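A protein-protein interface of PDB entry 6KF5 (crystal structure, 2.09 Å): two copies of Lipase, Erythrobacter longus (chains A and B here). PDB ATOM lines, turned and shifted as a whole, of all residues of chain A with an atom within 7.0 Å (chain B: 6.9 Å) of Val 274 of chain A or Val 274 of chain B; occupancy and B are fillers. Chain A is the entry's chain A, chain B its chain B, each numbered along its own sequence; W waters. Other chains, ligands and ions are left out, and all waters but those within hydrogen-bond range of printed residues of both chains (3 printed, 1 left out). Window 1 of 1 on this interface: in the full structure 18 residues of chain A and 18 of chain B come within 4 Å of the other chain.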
ATOM      1  N   PRO A 244      13.401  16.696  29.614  1.00  0.00           N
ATOM      2  CA  PRO A 244      12.245  17.556  29.355  1.00  0.00           C
ATOM      3  C   PRO A 244      11.090  16.743  28.797  1.00  0.00           C
ATOM      4  O   PRO A 244      11.274  15.561  28.453  1.00  0.00           O
ATOM      5  CB  PRO A 244      12.789  18.555  28.322  1.00  0.00           C
ATOM      6  CG  PRO A 244      13.894  17.797  27.611  1.00  0.00           C
ATOM      7  CD  PRO A 244      14.523  16.953  28.689  1.00  0.00           C
ATOM      8  N   PRO A 245       9.883  17.321  28.704  1.00  0.00           N
ATOM      9  CA  PRO A 245       8.786  16.617  28.015  1.00  0.00           C
ATOM     10  C   PRO A 245       9.245  16.199  26.622  1.00  0.00           C
ATOM     11  O   PRO A 245       9.972  16.936  25.955  1.00  0.00           O
ATOM     12  CB  PRO A 245       7.658  17.660  27.954  1.00  0.00           C
ATOM     13  CG  PRO A 245       7.990  18.674  29.023  1.00  0.00           C
ATOM     14  CD  PRO A 245       9.489  18.663  29.179  1.00  0.00           C
ATOM     15  N   THR A 246       8.835  14.999  26.192  1.00  0.00           N
ATOM     16  CA  THR A 246       9.415  14.371  25.011  1.00  0.00           C
ATOM     17  C   THR A 246       8.330  13.756  24.131  1.00  0.00           C
ATOM     18  O   THR A 246       7.350  13.199  24.637  1.00  0.00           O
ATOM     19  CB  THR A 246      10.434  13.279  25.410  1.00  0.00           C
ATOM     20  OG1 THR A 246      11.497  13.876  26.162  1.00  0.00           O
ATOM     21  CG2 THR A 246      11.030  12.573  24.162  1.00  0.00           C
ATOM     22  N   ILE A 247       8.513  13.869  22.815  1.00  0.00           N
ATOM     23  CA  ILE A 247       7.775  13.088  21.828  1.00  0.00           C
ATOM     24  C   ILE A 247       8.805  12.258  21.069  1.00  0.00           C
ATOM     25  O   ILE A 247       9.685  12.815  20.396  1.00  0.00           O
ATOM     26  CB  ILE A 247       6.962  13.975  20.872  1.00  0.00           C
ATOM     27  CG1 ILE A 247       5.907  14.762  21.660  1.00  0.00           C
ATOM     28  CG2 ILE A 247       6.284  13.116  19.765  1.00  0.00           C
ATOM     29  CD1 ILE A 247       5.438  16.002  20.967  1.00  0.00           C
ATOM     30  N   VAL A 248       8.733  10.940  21.211  1.00  0.00           N
ATOM     31  CA  VAL A 248       9.533  10.019  20.418  1.00  0.00           C
ATOM     32  C   VAL A 248       8.637   9.471  19.317  1.00  0.00           C
ATOM     33  O   VAL A 248       7.599   8.863  19.600  1.00  0.00           O
ATOM     34  CB  VAL A 248      10.106   8.870  21.262  1.00  0.00           C
ATOM     35  CG1 VAL A 248      10.950   7.951  20.388  1.00  0.00           C
ATOM     36  CG2 VAL A 248      10.929   9.393  22.463  1.00  0.00           C
ATOM     37  N   TYR A 263      14.605   4.233  24.017  1.00  0.00           N
ATOM     38  CA  TYR A 263      14.713   5.539  24.650  1.00  0.00           C
ATOM     39  C   TYR A 263      13.408   5.914  25.339  1.00  0.00           C
ATOM     40  O   TYR A 263      13.419   6.397  26.477  1.00  0.00           O
ATOM     41  CB  TYR A 263      15.117   6.608  23.635  1.00  0.00           C
ATOM     42  CG  TYR A 263      15.273   7.967  24.289  1.00  0.00           C
ATOM     43  CD1 TYR A 263      16.243   8.183  25.265  1.00  0.00           C
ATOM     44  CD2 TYR A 263      14.431   9.020  23.963  1.00  0.00           C
ATOM     45  CE1 TYR A 263      16.378   9.422  25.884  1.00  0.00           C
ATOM     46  CE2 TYR A 263      14.566  10.257  24.569  1.00  0.00           C
ATOM     47  CZ  TYR A 263      15.535  10.452  25.536  1.00  0.00           C
ATOM     48  OH  TYR A 263      15.665  11.686  26.149  1.00  0.00           O
ATOM     49  N   ALA A 264      12.273   5.684  24.672  1.00  0.00           N
ATOM     50  CA  ALA A 264      10.979   5.992  25.275  1.00  0.00           C
ATOM     51  C   ALA A 264      10.773   5.189  26.555  1.00  0.00           C
ATOM     52  O   ALA A 264      10.290   5.719  27.563  1.00  0.00           O
ATOM     53  CB  ALA A 264       9.848   5.710  24.278  1.00  0.00           C
ATOM     54  N   LYS A 265      11.143   3.909  26.535  1.00  0.00           N
ATOM     55  CA  LYS A 265      11.028   3.094  27.739  1.00  0.00           C
ATOM     56  C   LYS A 265      11.904   3.645  28.858  1.00  0.00           C
ATOM     57  O   LYS A 265      11.499   3.646  30.027  1.00  0.00           O
ATOM     58  CB  LYS A 265      11.399   1.642  27.431  1.00  0.00           C
ATOM     59  CG  LYS A 265      10.380   0.908  26.590  1.00  0.00           C
ATOM     60  CD  LYS A 265      10.925  -0.438  26.106  1.00  0.00           C
ATOM     61  CE  LYS A 265      11.093  -1.410  27.257  1.00  0.00           C
ATOM     62  NZ  LYS A 265      11.584  -2.762  26.814  1.00  0.00           N
ATOM     63  N   LEU A 267      12.649   6.748  29.373  1.00  0.00           N
ATOM     64  CA  LEU A 267      12.006   7.933  29.927  1.00  0.00           C
ATOM     65  C   LEU A 267      10.872   7.547  30.873  1.00  0.00           C
ATOM     66  O   LEU A 267      10.717   8.148  31.941  1.00  0.00           O
ATOM     67  CB  LEU A 267      11.499   8.818  28.791  1.00  0.00           C
ATOM     68  CG  LEU A 267      12.569   9.523  27.947  1.00  0.00           C
ATOM     69  CD1 LEU A 267      11.909  10.405  26.897  1.00  0.00           C
ATOM     70  CD2 LEU A 267      13.490  10.358  28.801  1.00  0.00           C
ATOM     71  N   VAL A 268      10.073   6.546  30.500  1.00  0.00           N
ATOM     72  CA  VAL A 268       9.023   6.054  31.393  1.00  0.00           C
ATOM     73  C   VAL A 268       9.634   5.512  32.683  1.00  0.00           C
ATOM     74  O   VAL A 268       9.183   5.837  33.787  1.00  0.00           O
ATOM     75  CB  VAL A 268       8.174   4.984  30.682  1.00  0.00           C
ATOM     76  CG1 VAL A 268       7.192   4.346  31.662  1.00  0.00           C
ATOM     77  CG2 VAL A 268       7.426   5.603  29.503  1.00  0.00           C
ATOM     78  N   GLY A 271      10.268   8.095  35.008  1.00  0.00           N
ATOM     79  CA  GLY A 271       9.144   8.920  35.419  1.00  0.00           C
ATOM     80  C   GLY A 271       8.947  10.203  34.638  1.00  0.00           C
ATOM     81  O   GLY A 271       8.327  11.139  35.156  1.00  0.00           O
ATOM     82  N   ARG A 272       9.459  10.285  33.410  1.00  0.00           N
ATOM     83  CA  ARG A 272       9.330  11.499  32.608  1.00  0.00           C
ATOM     84  C   ARG A 272       8.102  11.410  31.704  1.00  0.00           C
ATOM     85  O   ARG A 272       7.673  10.322  31.316  1.00  0.00           O
ATOM     86  CB  ARG A 272      10.588  11.715  31.767  1.00  0.00           C
ATOM     87  CG  ARG A 272      11.893  11.534  32.522  1.00  0.00           C
ATOM     88  CD  ARG A 272      11.913  12.364  33.798  1.00  0.00           C
ATOM     89  NE  ARG A 272      11.835  13.794  33.522  1.00  0.00           N
ATOM     90  CZ  ARG A 272      11.293  14.687  34.348  1.00  0.00           C
ATOM     91  NH1 ARG A 272      10.773  14.293  35.507  1.00  0.00           N
ATOM     92  NH2 ARG A 272      11.269  15.967  34.016  1.00  0.00           N
ATOM     93  N   ASP A 273       7.537  12.564  31.363  1.00  0.00           N
ATOM     94  CA  ASP A 273       6.391  12.591  30.464  1.00  0.00           C
ATOM     95  C   ASP A 273       6.849  12.346  29.031  1.00  0.00           C
ATOM     96  O   ASP A 273       7.746  13.041  28.548  1.00  0.00           O
ATOM     97  CB  ASP A 273       5.691  13.940  30.542  1.00  0.00           C
ATOM     98  CG  ASP A 273       5.101  14.222  31.905  1.00  0.00           C
ATOM     99  OD1 ASP A 273       4.961  13.284  32.730  1.00  0.00           O
ATOM    100  OD2 ASP A 273       4.774  15.400  32.132  1.00  0.00           O
ATOM    101  N   VAL A 274       6.229  11.383  28.335  1.00  0.00           N
ATOM    102  CA  VAL A 274       6.650  11.074  26.964  1.00  0.00           C
ATOM    103  C   VAL A 274       5.446  10.624  26.136  1.00  0.00           C
ATOM    104  O   VAL A 274       4.591   9.861  26.602  1.00  0.00           O
ATOM    105  CB  VAL A 274       7.794  10.023  26.939  1.00  0.00           C
ATOM    106  CG1 VAL A 274       7.406   8.757  27.667  1.00  0.00           C
ATOM    107  CG2 VAL A 274       8.193   9.680  25.499  1.00  0.00           C
ATOM    108  N   VAL A 275       5.359  11.139  24.908  1.00  0.00           N
ATOM    109  CA  VAL A 275       4.456  10.614  23.883  1.00  0.00           C
ATOM    110  C   VAL A 275       5.264   9.695  22.975  1.00  0.00           C
ATOM    111  O   VAL A 275       6.250  10.131  22.366  1.00  0.00           O
ATOM    112  CB  VAL A 275       3.809  11.735  23.054  1.00  0.00           C
ATOM    113  CG1 VAL A 275       2.830  11.112  22.044  1.00  0.00           C
ATOM    114  CG2 VAL A 275       3.119  12.789  23.947  1.00  0.00           C
ATOM    115  N   TYR A 276       4.874   8.431  22.888  1.00  0.00           N
ATOM    116  CA  TYR A 276       5.549   7.486  22.008  1.00  0.00           C
ATOM    117  C   TYR A 276       4.615   7.172  20.842  1.00  0.00           C
ATOM    118  O   TYR A 276       3.560   6.563  21.040  1.00  0.00           O
ATOM    119  CB  TYR A 276       5.961   6.204  22.735  1.00  0.00           C
ATOM    120  CG  TYR A 276       6.627   5.252  21.769  1.00  0.00           C
ATOM    121  CD1 TYR A 276       7.905   5.515  21.287  1.00  0.00           C
ATOM    122  CD2 TYR A 276       5.960   4.138  21.277  1.00  0.00           C
ATOM    123  CE1 TYR A 276       8.513   4.688  20.368  1.00  0.00           C
ATOM    124  CE2 TYR A 276       6.570   3.287  20.349  1.00  0.00           C
ATOM    125  CZ  TYR A 276       7.850   3.576  19.900  1.00  0.00           C
ATOM    126  OH  TYR A 276       8.473   2.756  18.978  1.00  0.00           O
ATOM    127  N   LEU A 277       5.009   7.572  19.628  1.00  0.00           N
ATOM    128  CA  LEU A 277       4.241   7.304  18.408  1.00  0.00           C
ATOM    129  C   LEU A 277       5.059   6.420  17.476  1.00  0.00           C
ATOM    130  O   LEU A 277       6.162   6.795  17.065  1.00  0.00           O
ATOM    131  CB  LEU A 277       3.859   8.607  17.693  1.00  0.00           C
ATOM    132  CG  LEU A 277       3.071   9.629  18.522  1.00  0.00           C
ATOM    133  CD1 LEU A 277       2.938  10.949  17.765  1.00  0.00           C
ATOM    134  CD2 LEU A 277       1.685   9.083  18.920  1.00  0.00           C
ATOM    135  N   GLU A 278       4.513   5.268  17.108  1.00  0.00           N
ATOM    136  CA  GLU A 278       5.187   4.355  16.190  1.00  0.00           C
ATOM    137  C   GLU A 278       4.330   4.262  14.929  1.00  0.00           C
ATOM    138  O   GLU A 278       3.256   3.653  14.946  1.00  0.00           O
ATOM    139  CB  GLU A 278       5.419   2.978  16.831  1.00  0.00           C
ATOM    140  CG  GLU A 278       6.163   1.996  15.916  1.00  0.00           C
ATOM    141  CD  GLU A 278       6.689   0.767  16.640  1.00  0.00           C
ATOM    142  OE1 GLU A 278       7.325   0.898  17.712  1.00  0.00           O
ATOM    143  OE2 GLU A 278       6.467  -0.345  16.125  1.00  0.00           O
ATOM    144  N   MET A 310       1.650  18.932  23.756  1.00  0.00           N
ATOM    145  CA  MET A 310       2.668  18.928  24.803  1.00  0.00           C
ATOM    146  C   MET A 310       3.148  20.331  25.147  1.00  0.00           C
ATOM    147  O   MET A 310       3.667  20.531  26.245  1.00  0.00           O
ATOM    148  CB  MET A 310       3.854  18.041  24.409  1.00  0.00           C
ATOM    149  CG  MET A 310       3.510  16.544  24.369  1.00  0.00           C
ATOM    150  SD  MET A 310       3.045  15.852  25.974  1.00  0.00           S
ATOM    151  CE  MET A 310       4.674  15.508  26.661  1.00  0.00           C
ATOM    152  N   PRO B 244      -5.018  -0.748  22.054  1.00  0.00           N
ATOM    153  CA  PRO B 244      -5.502   0.482  21.421  1.00  0.00           C
ATOM    154  C   PRO B 244      -4.634   1.658  21.828  1.00  0.00           C
ATOM    155  O   PRO B 244      -3.803   1.519  22.740  1.00  0.00           O
ATOM    156  CB  PRO B 244      -6.924   0.619  21.981  1.00  0.00           C
ATOM    157  CG  PRO B 244      -6.826  -0.015  23.342  1.00  0.00           C
ATOM    158  CD  PRO B 244      -5.864  -1.170  23.183  1.00  0.00           C
ATOM    159  N   PRO B 245      -4.774   2.814  21.169  1.00  0.00           N
ATOM    160  CA  PRO B 245      -4.094   4.029  21.645  1.00  0.00           C
ATOM    161  C   PRO B 245      -4.385   4.272  23.119  1.00  0.00           C
ATOM    162  O   PRO B 245      -5.532   4.177  23.565  1.00  0.00           O
ATOM    163  CB  PRO B 245      -4.684   5.138  20.767  1.00  0.00           C
ATOM    164  CG  PRO B 245      -5.132   4.425  19.495  1.00  0.00           C
ATOM    165  CD  PRO B 245      -5.545   3.040  19.927  1.00  0.00           C
ATOM    166  N   THR B 246      -3.341   4.616  23.872  1.00  0.00           N
ATOM    167  CA  THR B 246      -3.393   4.600  25.325  1.00  0.00           C
ATOM    168  C   THR B 246      -2.816   5.882  25.912  1.00  0.00           C
ATOM    169  O   THR B 246      -1.814   6.404  25.421  1.00  0.00           O
ATOM    170  CB  THR B 246      -2.612   3.371  25.870  1.00  0.00           C
ATOM    171  OG1 THR B 246      -3.196   2.176  25.343  1.00  0.00           O
ATOM    172  CG2 THR B 246      -2.645   3.312  27.395  1.00  0.00           C
ATOM    173  N   ILE B 247      -3.464   6.391  26.959  1.00  0.00           N
ATOM    174  CA  ILE B 247      -2.885   7.398  27.842  1.00  0.00           C
ATOM    175  C   ILE B 247      -2.773   6.756  29.217  1.00  0.00           C
ATOM    176  O   ILE B 247      -3.792   6.432  29.844  1.00  0.00           O
ATOM    177  CB  ILE B 247      -3.715   8.686  27.902  1.00  0.00           C
ATOM    178  CG1 ILE B 247      -3.813   9.324  26.513  1.00  0.00           C
ATOM    179  CG2 ILE B 247      -3.106   9.684  28.899  1.00  0.00           C
ATOM    180  CD1 ILE B 247      -4.960  10.297  26.404  1.00  0.00           C
ATOM    181  N   VAL B 248      -1.546   6.526  29.667  1.00  0.00           N
ATOM    182  CA  VAL B 248      -1.280   6.067  31.023  1.00  0.00           C
ATOM    183  C   VAL B 248      -0.943   7.295  31.853  1.00  0.00           C
ATOM    184  O   VAL B 248       0.008   8.020  31.543  1.00  0.00           O
ATOM    185  CB  VAL B 248      -0.139   5.039  31.076  1.00  0.00           C
ATOM    186  CG1 VAL B 248       0.047   4.562  32.503  1.00  0.00           C
ATOM    187  CG2 VAL B 248      -0.417   3.857  30.142  1.00  0.00           C
ATOM    188  N   TYR B 263       3.399  -0.821  32.739  1.00  0.00           N
ATOM    189  CA  TYR B 263       2.429  -1.013  31.667  1.00  0.00           C
ATOM    190  C   TYR B 263       2.758  -0.137  30.456  1.00  0.00           C
ATOM    191  O   TYR B 263       2.741  -0.609  29.311  1.00  0.00           O
ATOM    192  CB  TYR B 263       1.007  -0.738  32.166  1.00  0.00           C
ATOM    193  CG  TYR B 263      -0.007  -0.993  31.075  1.00  0.00           C
ATOM    194  CD1 TYR B 263      -0.128  -2.257  30.510  1.00  0.00           C
ATOM    195  CD2 TYR B 263      -0.796   0.028  30.569  1.00  0.00           C
ATOM    196  CE1 TYR B 263      -1.031  -2.508  29.486  1.00  0.00           C
ATOM    197  CE2 TYR B 263      -1.712  -0.215  29.545  1.00  0.00           C
ATOM    198  CZ  TYR B 263      -1.817  -1.487  29.009  1.00  0.00           C
ATOM    199  OH  TYR B 263      -2.700  -1.757  27.981  1.00  0.00           O
ATOM    200  N   ALA B 264       3.047   1.144  30.690  1.00  0.00           N
ATOM    201  CA  ALA B 264       3.427   2.036  29.597  1.00  0.00           C
ATOM    202  C   ALA B 264       4.663   1.522  28.864  1.00  0.00           C
ATOM    203  O   ALA B 264       4.707   1.534  27.630  1.00  0.00           O
ATOM    204  CB  ALA B 264       3.678   3.441  30.139  1.00  0.00           C
ATOM    205  N   LYS B 265       5.664   1.041  29.610  1.00  0.00           N
ATOM    206  CA  LYS B 265       6.844   0.434  28.991  1.00  0.00           C
ATOM    207  C   LYS B 265       6.482  -0.786  28.161  1.00  0.00           C
ATOM    208  O   LYS B 265       7.050  -0.998  27.082  1.00  0.00           O
ATOM    209  CB  LYS B 265       7.873   0.045  30.053  1.00  0.00           C
ATOM    210  CG  LYS B 265       8.564   1.237  30.680  1.00  0.00           C
ATOM    211  CD  LYS B 265       9.367   0.834  31.915  1.00  0.00           C
ATOM    212  CE  LYS B 265      10.656   0.117  31.525  1.00  0.00           C
ATOM    213  NZ  LYS B 265      11.384  -0.416  32.721  1.00  0.00           N
ATOM    214  N   LEU B 267       3.741  -1.279  26.588  1.00  0.00           N
ATOM    215  CA  LEU B 267       3.132  -0.804  25.351  1.00  0.00           C
ATOM    216  C   LEU B 267       4.195  -0.342  24.364  1.00  0.00           C
ATOM    217  O   LEU B 267       4.141  -0.709  23.189  1.00  0.00           O
ATOM    218  CB  LEU B 267       2.132   0.316  25.640  1.00  0.00           C
ATOM    219  CG  LEU B 267       0.900  -0.188  26.384  1.00  0.00           C
ATOM    220  CD1 LEU B 267      -0.090   0.933  26.650  1.00  0.00           C
ATOM    221  CD2 LEU B 267       0.248  -1.339  25.631  1.00  0.00           C
ATOM    222  N   VAL B 268       5.186   0.430  24.829  1.00  0.00           N
ATOM    223  CA  VAL B 268       6.280   0.840  23.948  1.00  0.00           C
ATOM    224  C   VAL B 268       7.020  -0.386  23.417  1.00  0.00           C
ATOM    225  O   VAL B 268       7.303  -0.493  22.218  1.00  0.00           O
ATOM    226  CB  VAL B 268       7.245   1.795  24.672  1.00  0.00           C
ATOM    227  CG1 VAL B 268       8.454   2.105  23.768  1.00  0.00           C
ATOM    228  CG2 VAL B 268       6.543   3.086  25.103  1.00  0.00           C
ATOM    229  N   ARG B 272       3.191   0.094  20.489  1.00  0.00           N
ATOM    230  CA  ARG B 272       1.880   0.727  20.500  1.00  0.00           C
ATOM    231  C   ARG B 272       2.003   2.201  20.869  1.00  0.00           C
ATOM    232  O   ARG B 272       2.892   2.597  21.621  1.00  0.00           O
ATOM    233  CB  ARG B 272       0.944   0.023  21.490  1.00  0.00           C
ATOM    234  CG  ARG B 272       1.035  -1.487  21.457  1.00  0.00           C
ATOM    235  CD  ARG B 272       0.774  -2.018  20.053  1.00  0.00           C
ATOM    236  NE  ARG B 272      -0.563  -1.661  19.591  1.00  0.00           N
ATOM    237  CZ  ARG B 272      -0.888  -1.482  18.312  1.00  0.00           C
ATOM    238  NH1 ARG B 272       0.032  -1.629  17.359  1.00  0.00           N
ATOM    239  NH2 ARG B 272      -2.134  -1.151  17.982  1.00  0.00           N
ATOM    240  N   ASP B 273       1.098   3.012  20.336  1.00  0.00           N
ATOM    241  CA  ASP B 273       1.118   4.435  20.645  1.00  0.00           C
ATOM    242  C   ASP B 273       0.652   4.663  22.082  1.00  0.00           C
ATOM    243  O   ASP B 273      -0.409   4.168  22.487  1.00  0.00           O
ATOM    244  CB  ASP B 273       0.224   5.201  19.670  1.00  0.00           C
ATOM    245  CG  ASP B 273       0.700   5.102  18.217  1.00  0.00           C
ATOM    246  OD1 ASP B 273       1.863   4.713  17.958  1.00  0.00           O
ATOM    247  OD2 ASP B 273      -0.106   5.411  17.329  1.00  0.00           O
ATOM    248  N   VAL B 274       1.427   5.423  22.855  1.00  0.00           N
ATOM    249  CA  VAL B 274       1.059   5.650  24.252  1.00  0.00           C
ATOM    250  C   VAL B 274       1.581   7.004  24.711  1.00  0.00           C
ATOM    251  O   VAL B 274       2.672   7.440  24.332  1.00  0.00           O
ATOM    252  CB  VAL B 274       1.559   4.501  25.165  1.00  0.00           C
ATOM    253  CG1 VAL B 274       3.024   4.170  24.904  1.00  0.00           C
ATOM    254  CG2 VAL B 274       1.335   4.844  26.650  1.00  0.00           C
ATOM    255  N   VAL B 275       0.757   7.690  25.493  1.00  0.00           N
ATOM    256  CA  VAL B 275       1.137   8.899  26.213  1.00  0.00           C
ATOM    257  C   VAL B 275       1.332   8.497  27.665  1.00  0.00           C
ATOM    258  O   VAL B 275       0.385   8.028  28.310  1.00  0.00           O
ATOM    259  CB  VAL B 275       0.059   9.998  26.109  1.00  0.00           C
ATOM    260  CG1 VAL B 275       0.528  11.277  26.824  1.00  0.00           C
ATOM    261  CG2 VAL B 275      -0.312  10.286  24.659  1.00  0.00           C
ATOM    262  N   TYR B 276       2.537   8.696  28.190  1.00  0.00           N
ATOM    263  CA  TYR B 276       2.810   8.462  29.604  1.00  0.00           C
ATOM    264  C   TYR B 276       2.904   9.815  30.305  1.00  0.00           C
ATOM    265  O   TYR B 276       3.730  10.657  29.936  1.00  0.00           O
ATOM    266  CB  TYR B 276       4.089   7.630  29.811  1.00  0.00           C
ATOM    267  CG  TYR B 276       4.341   7.377  31.280  1.00  0.00           C
ATOM    268  CD1 TYR B 276       3.548   6.481  31.990  1.00  0.00           C
ATOM    269  CD2 TYR B 276       5.318   8.083  31.974  1.00  0.00           C
ATOM    270  CE1 TYR B 276       3.729   6.278  33.343  1.00  0.00           C
ATOM    271  CE2 TYR B 276       5.512   7.878  33.338  1.00  0.00           C
ATOM    272  CZ  TYR B 276       4.711   6.973  34.013  1.00  0.00           C
ATOM    273  OH  TYR B 276       4.887   6.767  35.364  1.00  0.00           O
ATOM    274  N   LEU B 277       2.034  10.033  31.292  1.00  0.00           N
ATOM    275  CA  LEU B 277       2.027  11.253  32.092  1.00  0.00           C
ATOM    276  C   LEU B 277       2.180  10.870  33.556  1.00  0.00           C
ATOM    277  O   LEU B 277       1.331  10.167  34.111  1.00  0.00           O
ATOM    278  CB  LEU B 277       0.739  12.058  31.874  1.00  0.00           C
ATOM    279  CG  LEU B 277       0.448  12.479  30.423  1.00  0.00           C
ATOM    280  CD1 LEU B 277      -0.929  13.128  30.321  1.00  0.00           C
ATOM    281  CD2 LEU B 277       1.525  13.421  29.909  1.00  0.00           C
ATOM    282  N   GLU B 278       3.257  11.323  34.177  1.00  0.00           N
ATOM    283  CA  GLU B 278       3.491  11.087  35.595  1.00  0.00           C
ATOM    284  C   GLU B 278       3.374  12.437  36.306  1.00  0.00           C
ATOM    285  O   GLU B 278       4.249  13.293  36.169  1.00  0.00           O
ATOM    286  CB  GLU B 278       4.851  10.427  35.816  1.00  0.00           C
ATOM    287  CG  GLU B 278       5.146  10.129  37.272  1.00  0.00           C
ATOM    288  CD  GLU B 278       6.307   9.194  37.462  1.00  0.00           C
ATOM    289  OE1 GLU B 278       6.329   8.117  36.828  1.00  0.00           O
ATOM    290  OE2 GLU B 278       7.195   9.529  38.269  1.00  0.00           O
ATOM    291  N   MET B 310      -5.262  12.586  21.236  1.00  0.00           N
ATOM    292  CA  MET B 310      -5.196  11.195  20.816  1.00  0.00           C
ATOM    293  C   MET B 310      -6.460  10.758  20.084  1.00  0.00           C
ATOM    294  O   MET B 310      -6.442   9.734  19.392  1.00  0.00           O
ATOM    295  CB  MET B 310      -4.927  10.293  22.021  1.00  0.00           C
ATOM    296  CG  MET B 310      -3.523  10.430  22.587  1.00  0.00           C
ATOM    297  SD  MET B 310      -2.232   9.880  21.451  1.00  0.00           S
ATOM    298  CE  MET B 310      -2.295   8.091  21.648  1.00  0.00           C
HETATM  299  O   HOH W   1       0.400   4.513  14.766  1.00  0.00           O
HETATM  300  O   HOH W   2       4.498  16.016  34.890  1.00  0.00           O
HETATM  301  O   HOH W   3       1.812   1.991  16.699  1.00  0.00           O
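Ala 264 of chain A touches Val 268 of chain B (CB to CG1, 3.9 Å). Lys 265 of chain A touches Val 268 of chain B. Val 268 of chain A touches Lys 265 of chain B. Val 268 of chain A touches Tyr 276 of chain B. Asp 273 of chain A touches Tyr 276 of chain B. Val 275 of chain B touches Val 274 of chain A. CB of Tyr 276 of chain A touches CG2 of Val 268 of chain B, at 3.96 Å. CA of Asp 273 of chain B touches O of Tyr 276 of chain A, 3.3 Å away. OD1 of Asp 273 of chain B touches CA of Leu 277 of chain A, at 3.5 Å.
Lys 265 of chain A touches Val 268 of chain B, and with the chains exchanged Val 268 of chain A touches Lys 265 of chain B. Arg 272 of chain A touches Tyr 276 of chain B, and with the chains exchanged Tyr 276 of chain A touches Arg 272 of chain B. Asp 273 of chain A touches Leu 277 of chain B, and with the chains exchanged Leu 277 of chain A touches Asp 273 of chain B. Of the 21 pairs that touch across the chains among the printed residues, 20 have their exchanged pair printed and touching as well.
The side-chain carboxylate (OD1) of Asp 273 of chain A sits at hydrogen-bond distance from the backbone NH (N) of Glu 278 of chain B. The backbone carbonyl oxygen (O) of Val 274 of chain A is in hydrogen-bond range of the backbone NH (N) of Tyr 276 of chain B, at 2.8 Å. N of Tyr 276 of chain A is in hydrogen-bond range of O of Val 274 of chain B, at 2.8 Å. The backbone NH (N) of Glu 278 of chain A sits at hydrogen-bond distance from the side-chain carboxylate (OD1) of Asp 273 of chain B (2.8 Å).
Of the 19 printed residues of chain A, 11 touch a printed residue of chain B. Printed residues of chain A that touch a printed residue of chain B: Ala 264, Lys 265, Val 268, Gly 271, Arg 272, Asp 273, Val 274, Val 275, Tyr 276, Leu 277 and Glu 278. Of the 18 printed residues of chain B, 10 touch a printed residue of chain A. Printed residues of chain B that touch a printed residue of chain A: Ala 264, Lys 265, Val 268, Arg 272, Asp 273, Val 274, Val 275, Tyr 276, Leu 277 and Glu 278. Hydrophobic or aromatic side chains of chain B that line the printed part of chain A: Ala 264, Val 268 and Tyr 276.
O of Val 248 of chain A lies within hydrogen-bond range of N of Leu 277 of chain A, 2.9 Å away. The side-chain hydroxyl of Tyr 276 of chain A is in hydrogen-bond range of the side-chain carboxylate of Glu 278 of chain A (2.5 Å). The backbone NH (N) of Val 275 of chain B sits at hydrogen-bond distance from the backbone carbonyl oxygen (O) of Thr 246 of chain B (2.9 Å). The backbone carbonyl oxygen of Val 275 of chain B sits at hydrogen-bond distance from the backbone NH of Val 248 of chain B, 2.8 Å away.
Water W1 bridges the side-chain carboxylate of Asp 273 of chain B and the backbone carbonyl oxygen of Glu 278 of chain A. Water W3 bridges the backbone carbonyl oxygen of Glu 278 of chain A (2.8 Å) and the side-chain carboxylate of Asp 273 of chain B (3.0 Å). Water W2 lies within hydrogen-bond range of OD2 of Asp 273 of chain A (2.8 Å) and O of Glu 278 of chain B (3.0 Å).
Val 274 of chain A touches three residues of chain B. Val 274 of chain B touches just these residues of chain A: Val 274, Val 275 and Tyr 276. Of the printed residues of chain A, Val 275 of chain B touches Val 274. Printed residues of chain B within 4 Å of Asp 273 of chain A: Tyr 276, Leu 277 and Glu 278. Of the printed residues of chain A, Glu 278 of chain B touches Gly 271 (3.2 Å) and Asp 273 (3.0 Å). The nearest residue of chain B that does not touch Val 274 of chain A is Leu 277 of chain B (5.3 Å). The nearest printed residue of chain A that does not touch Leu 277 of chain B is Met 310 of chain A (4.9 Å).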
